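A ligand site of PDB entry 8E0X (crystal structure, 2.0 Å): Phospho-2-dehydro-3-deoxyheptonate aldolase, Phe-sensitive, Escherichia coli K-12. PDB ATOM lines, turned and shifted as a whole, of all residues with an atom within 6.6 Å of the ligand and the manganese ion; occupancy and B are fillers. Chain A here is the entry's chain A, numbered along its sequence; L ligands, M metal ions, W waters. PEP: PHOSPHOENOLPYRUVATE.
The side-chain amino group (NZ) of Lys 98 is in salt-bridge range of an oxygen (O1) of the ligand (2.9 Å). The backbone NH of Ala 165 is in hydrogen-bond range of an oxygen (O3P) of the ligand (3.1 Å). The guanidinium group (NH2) of Arg 93 is in salt-bridge range of an oxygen (O1) of the ligand, 2.8 Å away. An oxygen (O1P) of the ligand is in salt-bridge range of the guanidinium group of Arg 166, 2.9 Å away. NZ of Lys 187 is in salt-bridge range of O2P of the ligand (2.8 Å). An oxygen (O2P) of the ligand is in salt-bridge range of the guanidinium group (NE) of Arg 235. A ring nitrogen (NE2) of His 269 lies close to an oxygen (O2) of the ligand (3.3 Å).
The backbone NH of Arg 235 is in hydrogen-bond range of the side-chain amide oxygen of Asn 188. The guanidinium group (NH2) of Arg 93 sits at hydrogen-bond distance from the backbone carbonyl oxygen (O) of Cys 62, at 3.2 Å. The backbone NH of Ala 270 lies close to the backbone carbonyl oxygen of Arg 235, 3.4 Å away. SG of Cys 62 sits at hydrogen-bond distance from OG1 of Thr 326 (3.0 Å). The side-chain amino group of Lys 98 lies within hydrogen-bond range of the backbone carbonyl oxygen of Cys 62, 3.1 Å away. A ring nitrogen (ND1) of His 269 is in hydrogen-bond range of the side-chain carboxylate of Asp 266 (2.5 Å). The backbone NH (N) of Asp 327 sits at hydrogen-bond distance from the side-chain sulfur (SG) of Cys 62, 3.4 Å away. NZ of Lys 187 lies within salt-bridge range of OD2 of Asp 266, at 2.8 Å.
The side-chain carboxylate of Glu 144 lies close to an oxygen (O1) of the ligand, at 3.2 Å. Tyr 95 touches the ligand (CE2 to O1, 3.3 Å). Pro 99 touches the ligand. CA of Gly 164 touches O3P of the ligand, at 3.4 Å. Met 301 touches the ligand (SD to O2', 3.97 Å). Within 4 Å of the ligand: Arg 93, Tyr 95, Lys 98, Pro 99, Glu 144, Gly 164, Ala 165, Arg 166, Lys 187, Arg 235, His 269 and Met 301.
Of the 25 residues printed, 4 come within 4 Å of the manganese ion. The nearest printed residue that does not touch the manganese ion is Arg 93 (4.01 Å).
The manganese ion is bound by the side-chain carboxylate of Glu 303 (2.1 Å), the side-chain carboxylate of Asp 327 (2.3 Å) and a ring nitrogen (NE2) of His 269 (2.7 Å). Slightly farther from the manganese ion lies SG of Cys 62 (3.0 Å).
Water W3 lies within hydrogen-bond range of O1P of the ligand (2.4 Å) and NH2 of Arg 166 (2.9 Å). Water W2 lies within hydrogen-bond range of an oxygen (O2') of the ligand (2.5 Å), the side-chain hydroxyl (OH) of Tyr 95 (2.8 Å) and the side-chain sulfur (SD) of Met 301 (3.6 Å). Water W1 lies within hydrogen-bond range of NH1 of Arg 166, N of Ala 165 and O3P of the ligand.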
ATOM      1  N   CYS A  62     -17.732  17.004 -34.187  1.00  0.00           N
ATOM      2  CA  CYS A  62     -17.797  15.611 -33.767  1.00  0.00           C
ATOM      3  C   CYS A  62     -16.986  14.743 -34.704  1.00  0.00           C
ATOM      4  O   CYS A  62     -16.205  13.882 -34.268  1.00  0.00           O
ATOM      5  CB  CYS A  62     -19.243  15.133 -33.711  1.00  0.00           C
ATOM      6  SG  CYS A  62     -19.476  13.303 -33.641  1.00  0.00           S
ATOM      7  N   SER A  63     -17.134  14.967 -36.007  1.00  0.00           N
ATOM      8  CA  SER A  63     -16.400  14.230 -37.022  1.00  0.00           C
ATOM      9  C   SER A  63     -16.178  15.132 -38.230  1.00  0.00           C
ATOM     10  O   SER A  63     -17.021  15.970 -38.559  1.00  0.00           O
ATOM     11  CB  SER A  63     -17.159  12.982 -37.455  1.00  0.00           C
ATOM     12  OG  SER A  63     -18.387  13.334 -38.079  1.00  0.00           O
ATOM     13  N   ARG A  93     -10.226  19.668 -32.426  1.00  0.00           N
ATOM     14  CA  ARG A  93     -10.713  18.315 -32.575  1.00  0.00           C
ATOM     15  C   ARG A  93     -10.777  17.949 -34.058  1.00  0.00           C
ATOM     16  O   ARG A  93     -11.566  18.518 -34.809  1.00  0.00           O
ATOM     17  CB  ARG A  93     -12.088  18.269 -31.898  1.00  0.00           C
ATOM     18  CG  ARG A  93     -12.742  16.974 -31.789  1.00  0.00           C
ATOM     19  CD  ARG A  93     -13.991  17.130 -30.972  1.00  0.00           C
ATOM     20  NE  ARG A  93     -14.946  16.105 -31.344  1.00  0.00           N
ATOM     21  CZ  ARG A  93     -15.220  15.037 -30.607  1.00  0.00           C
ATOM     22  NH1 ARG A  93     -14.718  14.876 -29.396  1.00  0.00           N
ATOM     23  NH2 ARG A  93     -16.027  14.106 -31.112  1.00  0.00           N
ATOM     24  N   TYR A  95     -11.395  14.611 -35.774  1.00  0.00           N
ATOM     25  CA  TYR A  95     -11.744  13.166 -35.646  1.00  0.00           C
ATOM     26  C   TYR A  95     -12.277  12.593 -36.949  1.00  0.00           C
ATOM     27  O   TYR A  95     -13.295  13.074 -37.445  1.00  0.00           O
ATOM     28  CB  TYR A  95     -12.811  13.017 -34.569  1.00  0.00           C
ATOM     29  CG  TYR A  95     -12.366  13.128 -33.131  1.00  0.00           C
ATOM     30  CD1 TYR A  95     -11.243  13.862 -32.775  1.00  0.00           C
ATOM     31  CD2 TYR A  95     -13.085  12.503 -32.118  1.00  0.00           C
ATOM     32  CE1 TYR A  95     -10.847  13.962 -31.456  1.00  0.00           C
ATOM     33  CE2 TYR A  95     -12.690  12.593 -30.796  1.00  0.00           C
ATOM     34  CZ  TYR A  95     -11.565  13.332 -30.465  1.00  0.00           C
ATOM     35  OH  TYR A  95     -11.170  13.416 -29.165  1.00  0.00           O
ATOM     36  N   LYS A  98     -14.690   7.214 -36.279  1.00  0.00           N
ATOM     37  CA  LYS A  98     -15.790   7.179 -35.275  1.00  0.00           C
ATOM     38  C   LYS A  98     -16.101   5.785 -34.725  1.00  0.00           C
ATOM     39  O   LYS A  98     -16.173   4.824 -35.512  1.00  0.00           O
ATOM     40  CB  LYS A  98     -17.029   7.829 -35.895  1.00  0.00           C
ATOM     41  CG  LYS A  98     -16.830   9.272 -36.345  1.00  0.00           C
ATOM     42  CD  LYS A  98     -16.313  10.145 -35.233  1.00  0.00           C
ATOM     43  CE  LYS A  98     -17.294  10.273 -34.080  1.00  0.00           C
ATOM     44  NZ  LYS A  98     -16.734  11.075 -32.967  1.00  0.00           N
ATOM     45  N   PRO A  99     -16.288   5.634 -33.392  1.00  0.00           N
ATOM     46  CA  PRO A  99     -16.727   4.364 -32.827  1.00  0.00           C
ATOM     47  C   PRO A  99     -18.269   4.272 -32.895  1.00  0.00           C
ATOM     48  O   PRO A  99     -18.916   5.191 -32.487  1.00  0.00           O
ATOM     49  CB  PRO A  99     -16.275   4.502 -31.359  1.00  0.00           C
ATOM     50  CG  PRO A  99     -16.394   5.977 -31.083  1.00  0.00           C
ATOM     51  CD  PRO A  99     -16.050   6.662 -32.384  1.00  0.00           C
ATOM     52  N   GLU A 144      -9.039  10.789 -32.119  1.00  0.00           N
ATOM     53  CA  GLU A 144      -9.426   9.582 -31.356  1.00  0.00           C
ATOM     54  C   GLU A 144      -8.644   8.410 -31.944  1.00  0.00           C
ATOM     55  O   GLU A 144      -8.602   8.303 -33.165  1.00  0.00           O
ATOM     56  CB  GLU A 144     -10.932   9.330 -31.441  1.00  0.00           C
ATOM     57  CG  GLU A 144     -11.532   8.687 -30.213  1.00  0.00           C
ATOM     58  CD  GLU A 144     -13.042   8.880 -30.130  1.00  0.00           C
ATOM     59  OE1 GLU A 144     -13.655   9.126 -31.180  1.00  0.00           O
ATOM     60  OE2 GLU A 144     -13.582   8.783 -29.022  1.00  0.00           O
ATOM     61  N   ALA A 162      -7.444  10.817 -27.681  1.00  0.00           N
ATOM     62  CA  ALA A 162      -8.463  10.254 -26.784  1.00  0.00           C
ATOM     63  C   ALA A 162      -8.693   8.776 -27.094  1.00  0.00           C
ATOM     64  O   ALA A 162      -8.730   8.420 -28.278  1.00  0.00           O
ATOM     65  CB  ALA A 162      -9.752  11.004 -26.942  1.00  0.00           C
ATOM     66  N   ILE A 163      -8.802   7.953 -26.058  1.00  0.00           N
ATOM     67  CA  ILE A 163      -9.213   6.548 -26.267  1.00  0.00           C
ATOM     68  C   ILE A 163     -10.713   6.575 -25.972  1.00  0.00           C
ATOM     69  O   ILE A 163     -11.090   7.062 -24.920  1.00  0.00           O
ATOM     70  CB  ILE A 163      -8.453   5.574 -25.357  1.00  0.00           C
ATOM     71  CG1 ILE A 163      -6.952   5.579 -25.651  1.00  0.00           C
ATOM     72  CG2 ILE A 163      -9.040   4.175 -25.436  1.00  0.00           C
ATOM     73  CD1 ILE A 163      -6.592   5.124 -27.036  1.00  0.00           C
ATOM     74  N   GLY A 164     -11.516   6.044 -26.875  1.00  0.00           N
ATOM     75  CA  GLY A 164     -12.953   6.119 -26.707  1.00  0.00           C
ATOM     76  C   GLY A 164     -13.444   5.305 -25.524  1.00  0.00           C
ATOM     77  O   GLY A 164     -12.836   4.317 -25.100  1.00  0.00           O
ATOM     78  N   ALA A 165     -14.599   5.725 -24.993  1.00  0.00           N
ATOM     79  CA  ALA A 165     -15.221   5.047 -23.872  1.00  0.00           C
ATOM     80  C   ALA A 165     -15.388   3.559 -24.132  1.00  0.00           C
ATOM     81  O   ALA A 165     -15.260   2.745 -23.209  1.00  0.00           O
ATOM     82  CB  ALA A 165     -16.583   5.669 -23.567  1.00  0.00           C
ATOM     83  N   ARG A 166     -15.653   3.178 -25.383  1.00  0.00           N
ATOM     84  CA  ARG A 166     -15.898   1.781 -25.720  1.00  0.00           C
ATOM     85  C   ARG A 166     -14.628   0.930 -25.680  1.00  0.00           C
ATOM     86  O   ARG A 166     -14.737  -0.300 -25.715  1.00  0.00           O
ATOM     87  CB  ARG A 166     -16.550   1.701 -27.115  1.00  0.00           C
ATOM     88  CG  ARG A 166     -18.027   2.082 -27.094  1.00  0.00           C
ATOM     89  CD  ARG A 166     -18.588   2.465 -28.467  1.00  0.00           C
ATOM     90  NE  ARG A 166     -19.839   3.212 -28.327  1.00  0.00           N
ATOM     91  CZ  ARG A 166     -19.919   4.504 -28.034  1.00  0.00           C
ATOM     92  NH1 ARG A 166     -18.838   5.266 -27.927  1.00  0.00           N
ATOM     93  NH2 ARG A 166     -21.113   5.057 -27.826  1.00  0.00           N
ATOM     94  N   LYS A 187     -11.599   8.108 -21.594  1.00  0.00           N
ATOM     95  CA  LYS A 187     -12.974   8.373 -21.175  1.00  0.00           C
ATOM     96  C   LYS A 187     -13.430   7.342 -20.155  1.00  0.00           C
ATOM     97  O   LYS A 187     -13.098   6.156 -20.253  1.00  0.00           O
ATOM     98  CB  LYS A 187     -13.882   8.380 -22.394  1.00  0.00           C
ATOM     99  CG  LYS A 187     -14.005   9.769 -23.012  1.00  0.00           C
ATOM    100  CD  LYS A 187     -14.290   9.723 -24.483  1.00  0.00           C
ATOM    101  CE  LYS A 187     -14.482  11.131 -25.038  1.00  0.00           C
ATOM    102  NZ  LYS A 187     -15.879  11.621 -24.906  1.00  0.00           N
ATOM    103  N   ASN A 188     -14.256   7.812 -19.224  1.00  0.00           N
ATOM    104  CA  ASN A 188     -14.921   6.872 -18.293  1.00  0.00           C
ATOM    105  C   ASN A 188     -15.816   5.956 -19.128  1.00  0.00           C
ATOM    106  O   ASN A 188     -16.063   6.268 -20.290  1.00  0.00           O
ATOM    107  CB  ASN A 188     -15.672   7.604 -17.189  1.00  0.00           C
ATOM    108  CG  ASN A 188     -16.802   8.478 -17.677  1.00  0.00           C
ATOM    109  OD1 ASN A 188     -16.724   9.702 -17.608  1.00  0.00           O
ATOM    110  ND2 ASN A 188     -17.867   7.866 -18.165  1.00  0.00           N
ATOM    111  N   THR A 190     -18.941   3.797 -20.844  1.00  0.00           N
ATOM    112  CA  THR A 190     -20.211   4.253 -21.386  1.00  0.00           C
ATOM    113  C   THR A 190     -21.347   4.253 -20.354  1.00  0.00           C
ATOM    114  O   THR A 190     -22.360   4.925 -20.559  1.00  0.00           O
ATOM    115  CB  THR A 190     -20.631   3.426 -22.605  1.00  0.00           C
ATOM    116  OG1 THR A 190     -20.574   2.033 -22.297  1.00  0.00           O
ATOM    117  CG2 THR A 190     -19.742   3.753 -23.821  1.00  0.00           C
ATOM    118  N   ARG A 235     -17.147  12.069 -19.052  1.00  0.00           N
ATOM    119  CA  ARG A 235     -18.002  12.111 -20.220  1.00  0.00           C
ATOM    120  C   ARG A 235     -19.444  11.764 -19.899  1.00  0.00           C
ATOM    121  O   ARG A 235     -20.258  11.693 -20.823  1.00  0.00           O
ATOM    122  CB  ARG A 235     -17.508  11.130 -21.300  1.00  0.00           C
ATOM    123  CG  ARG A 235     -17.822   9.689 -20.891  1.00  0.00           C
ATOM    124  CD  ARG A 235     -17.807   8.723 -22.035  1.00  0.00           C
ATOM    125  NE  ARG A 235     -18.905   8.890 -22.987  1.00  0.00           N
ATOM    126  CZ  ARG A 235     -20.117   8.357 -22.843  1.00  0.00           C
ATOM    127  NH1 ARG A 235     -20.455   7.699 -21.753  1.00  0.00           N
ATOM    128  NH2 ARG A 235     -21.004   8.495 -23.824  1.00  0.00           N
ATOM    129  N   ASP A 266     -15.655  16.550 -20.590  1.00  0.00           N
ATOM    130  CA  ASP A 266     -16.337  16.598 -21.881  1.00  0.00           C
ATOM    131  C   ASP A 266     -17.710  17.218 -21.676  1.00  0.00           C
ATOM    132  O   ASP A 266     -18.513  16.698 -20.893  1.00  0.00           O
ATOM    133  CB  ASP A 266     -16.431  15.190 -22.466  1.00  0.00           C
ATOM    134  CG  ASP A 266     -17.090  15.126 -23.846  1.00  0.00           C
ATOM    135  OD1 ASP A 266     -17.478  16.171 -24.411  1.00  0.00           O
ATOM    136  OD2 ASP A 266     -17.212  14.012 -24.376  1.00  0.00           O
ATOM    137  N   SER A 268     -20.017  17.389 -23.844  1.00  0.00           N
ATOM    138  CA  SER A 268     -20.943  16.816 -24.798  1.00  0.00           C
ATOM    139  C   SER A 268     -21.336  15.390 -24.390  1.00  0.00           C
ATOM    140  O   SER A 268     -21.267  15.036 -23.202  1.00  0.00           O
ATOM    141  CB  SER A 268     -20.289  16.880 -26.190  1.00  0.00           C
ATOM    142  OG  SER A 268     -21.270  16.785 -27.209  1.00  0.00           O
ATOM    143  N   HIS A 269     -21.741  14.582 -25.368  1.00  0.00           N
ATOM    144  CA  HIS A 269     -22.050  13.148 -25.210  1.00  0.00           C
ATOM    145  C   HIS A 269     -22.998  12.995 -24.018  1.00  0.00           C
ATOM    146  O   HIS A 269     -23.979  13.734 -23.907  1.00  0.00           O
ATOM    147  CB  HIS A 269     -20.754  12.356 -25.129  1.00  0.00           C
ATOM    148  CG  HIS A 269     -19.855  12.551 -26.315  1.00  0.00           C
ATOM    149  ND1 HIS A 269     -18.698  13.306 -26.261  1.00  0.00           N
ATOM    150  CD2 HIS A 269     -19.928  12.085 -27.586  1.00  0.00           C
ATOM    151  CE1 HIS A 269     -18.108  13.300 -27.445  1.00  0.00           C
ATOM    152  NE2 HIS A 269     -18.839  12.565 -28.270  1.00  0.00           N
ATOM    153  N   ALA A 270     -22.737  12.059 -23.097  1.00  0.00           N
ATOM    154  CA  ALA A 270     -23.662  11.816 -21.991  1.00  0.00           C
ATOM    155  C   ALA A 270     -23.697  12.951 -20.980  1.00  0.00           C
ATOM    156  O   ALA A 270     -24.602  12.968 -20.151  1.00  0.00           O
ATOM    157  CB  ALA A 270     -23.309  10.500 -21.286  1.00  0.00           C
ATOM    158  N   MET A 301     -13.528  19.455 -23.282  1.00  0.00           N
ATOM    159  CA  MET A 301     -13.727  19.018 -24.655  1.00  0.00           C
ATOM    160  C   MET A 301     -15.116  19.468 -25.068  1.00  0.00           C
ATOM    161  O   MET A 301     -16.073  19.321 -24.304  1.00  0.00           O
ATOM    162  CB  MET A 301     -13.564  17.488 -24.791  1.00  0.00           C
ATOM    163  CG  MET A 301     -14.046  16.853 -26.127  1.00  0.00           C
ATOM    164  SD  MET A 301     -13.878  15.024 -26.113  1.00  0.00           S
ATOM    165  CE  MET A 301     -12.116  14.905 -25.762  1.00  0.00           C
ATOM    166  N   GLU A 303     -17.907  19.938 -28.548  1.00  0.00           N
ATOM    167  CA  GLU A 303     -18.266  19.598 -29.913  1.00  0.00           C
ATOM    168  C   GLU A 303     -18.879  20.830 -30.574  1.00  0.00           C
ATOM    169  O   GLU A 303     -19.963  21.283 -30.185  1.00  0.00           O
ATOM    170  CB  GLU A 303     -19.212  18.397 -29.951  1.00  0.00           C
ATOM    171  CG  GLU A 303     -18.516  17.108 -29.524  1.00  0.00           C
ATOM    172  CD  GLU A 303     -19.325  15.878 -29.847  1.00  0.00           C
ATOM    173  OE1 GLU A 303     -20.558  15.908 -29.659  1.00  0.00           O
ATOM    174  OE2 GLU A 303     -18.743  14.867 -30.293  1.00  0.00           O
ATOM    175  N   THR A 326     -22.633  13.621 -37.972  1.00  0.00           N
ATOM    176  CA  THR A 326     -22.716  12.701 -36.849  1.00  0.00           C
ATOM    177  C   THR A 326     -23.425  13.444 -35.714  1.00  0.00           C
ATOM    178  O   THR A 326     -24.555  13.882 -35.896  1.00  0.00           O
ATOM    179  CB  THR A 326     -21.350  12.126 -36.487  1.00  0.00           C
ATOM    180  OG1 THR A 326     -20.362  13.160 -36.496  1.00  0.00           O
ATOM    181  CG2 THR A 326     -20.959  11.016 -37.456  1.00  0.00           C
ATOM    182  N   ASP A 327     -22.783  13.609 -34.560  1.00  0.00           N
ATOM    183  CA  ASP A 327     -23.454  14.192 -33.405  1.00  0.00           C
ATOM    184  C   ASP A 327     -23.660  15.691 -33.582  1.00  0.00           C
ATOM    185  O   ASP A 327     -22.899  16.368 -34.279  1.00  0.00           O
ATOM    186  CB  ASP A 327     -22.671  13.919 -32.131  1.00  0.00           C
ATOM    187  CG  ASP A 327     -22.756  12.475 -31.679  1.00  0.00           C
ATOM    188  OD1 ASP A 327     -23.748  11.793 -32.018  1.00  0.00           O
ATOM    189  OD2 ASP A 327     -21.826  12.011 -30.985  1.00  0.00           O
ATOM    190  N   ALA A 328     -24.691  16.217 -32.915  1.00  0.00           N
ATOM    191  CA  ALA A 328     -24.985  17.641 -33.004  1.00  0.00           C
ATOM    192  C   ALA A 328     -23.922  18.465 -32.271  1.00  0.00           C
ATOM    193  O   ALA A 328     -23.420  18.062 -31.223  1.00  0.00           O
ATOM    194  CB  ALA A 328     -26.376  17.944 -32.452  1.00  0.00           C
HETATM  195  C1  PEP L   1     -15.799  11.209 -29.062  1.00  0.00           C
HETATM  196  O1  PEP L   1     -15.674  11.413 -30.280  1.00  0.00           O
HETATM  197  O2' PEP L   1     -15.336  11.984 -28.208  1.00  0.00           O
HETATM  198  C2  PEP L   1     -16.535  10.035 -28.635  1.00  0.00           C
HETATM  199  C3  PEP L   1     -16.708   9.029 -29.473  1.00  0.00           C
HETATM  200  O2  PEP L   1     -17.101   9.983 -27.295  1.00  0.00           O
HETATM  201  P   PEP L   1     -17.114   8.649 -26.413  1.00  0.00           P
HETATM  202  O1P PEP L   1     -18.323   7.901 -26.882  1.00  0.00           O
HETATM  203  O2P PEP L   1     -17.254   9.188 -25.022  1.00  0.00           O
HETATM  204  O3P PEP L   1     -15.824   7.939 -26.701  1.00  0.00           O
HETATM  205 MN    MN M   1     -19.902  13.188 -30.666  1.00  0.00          MN
HETATM  206  O   HOH W   1     -16.121   4.835 -27.765  1.00  0.00           O
HETATM  207  O   HOH W   2     -12.923  11.899 -27.561  1.00  0.00           O
HETATM  208  O   HOH W   3     -20.572   7.914 -27.845  1.00  0.00           O
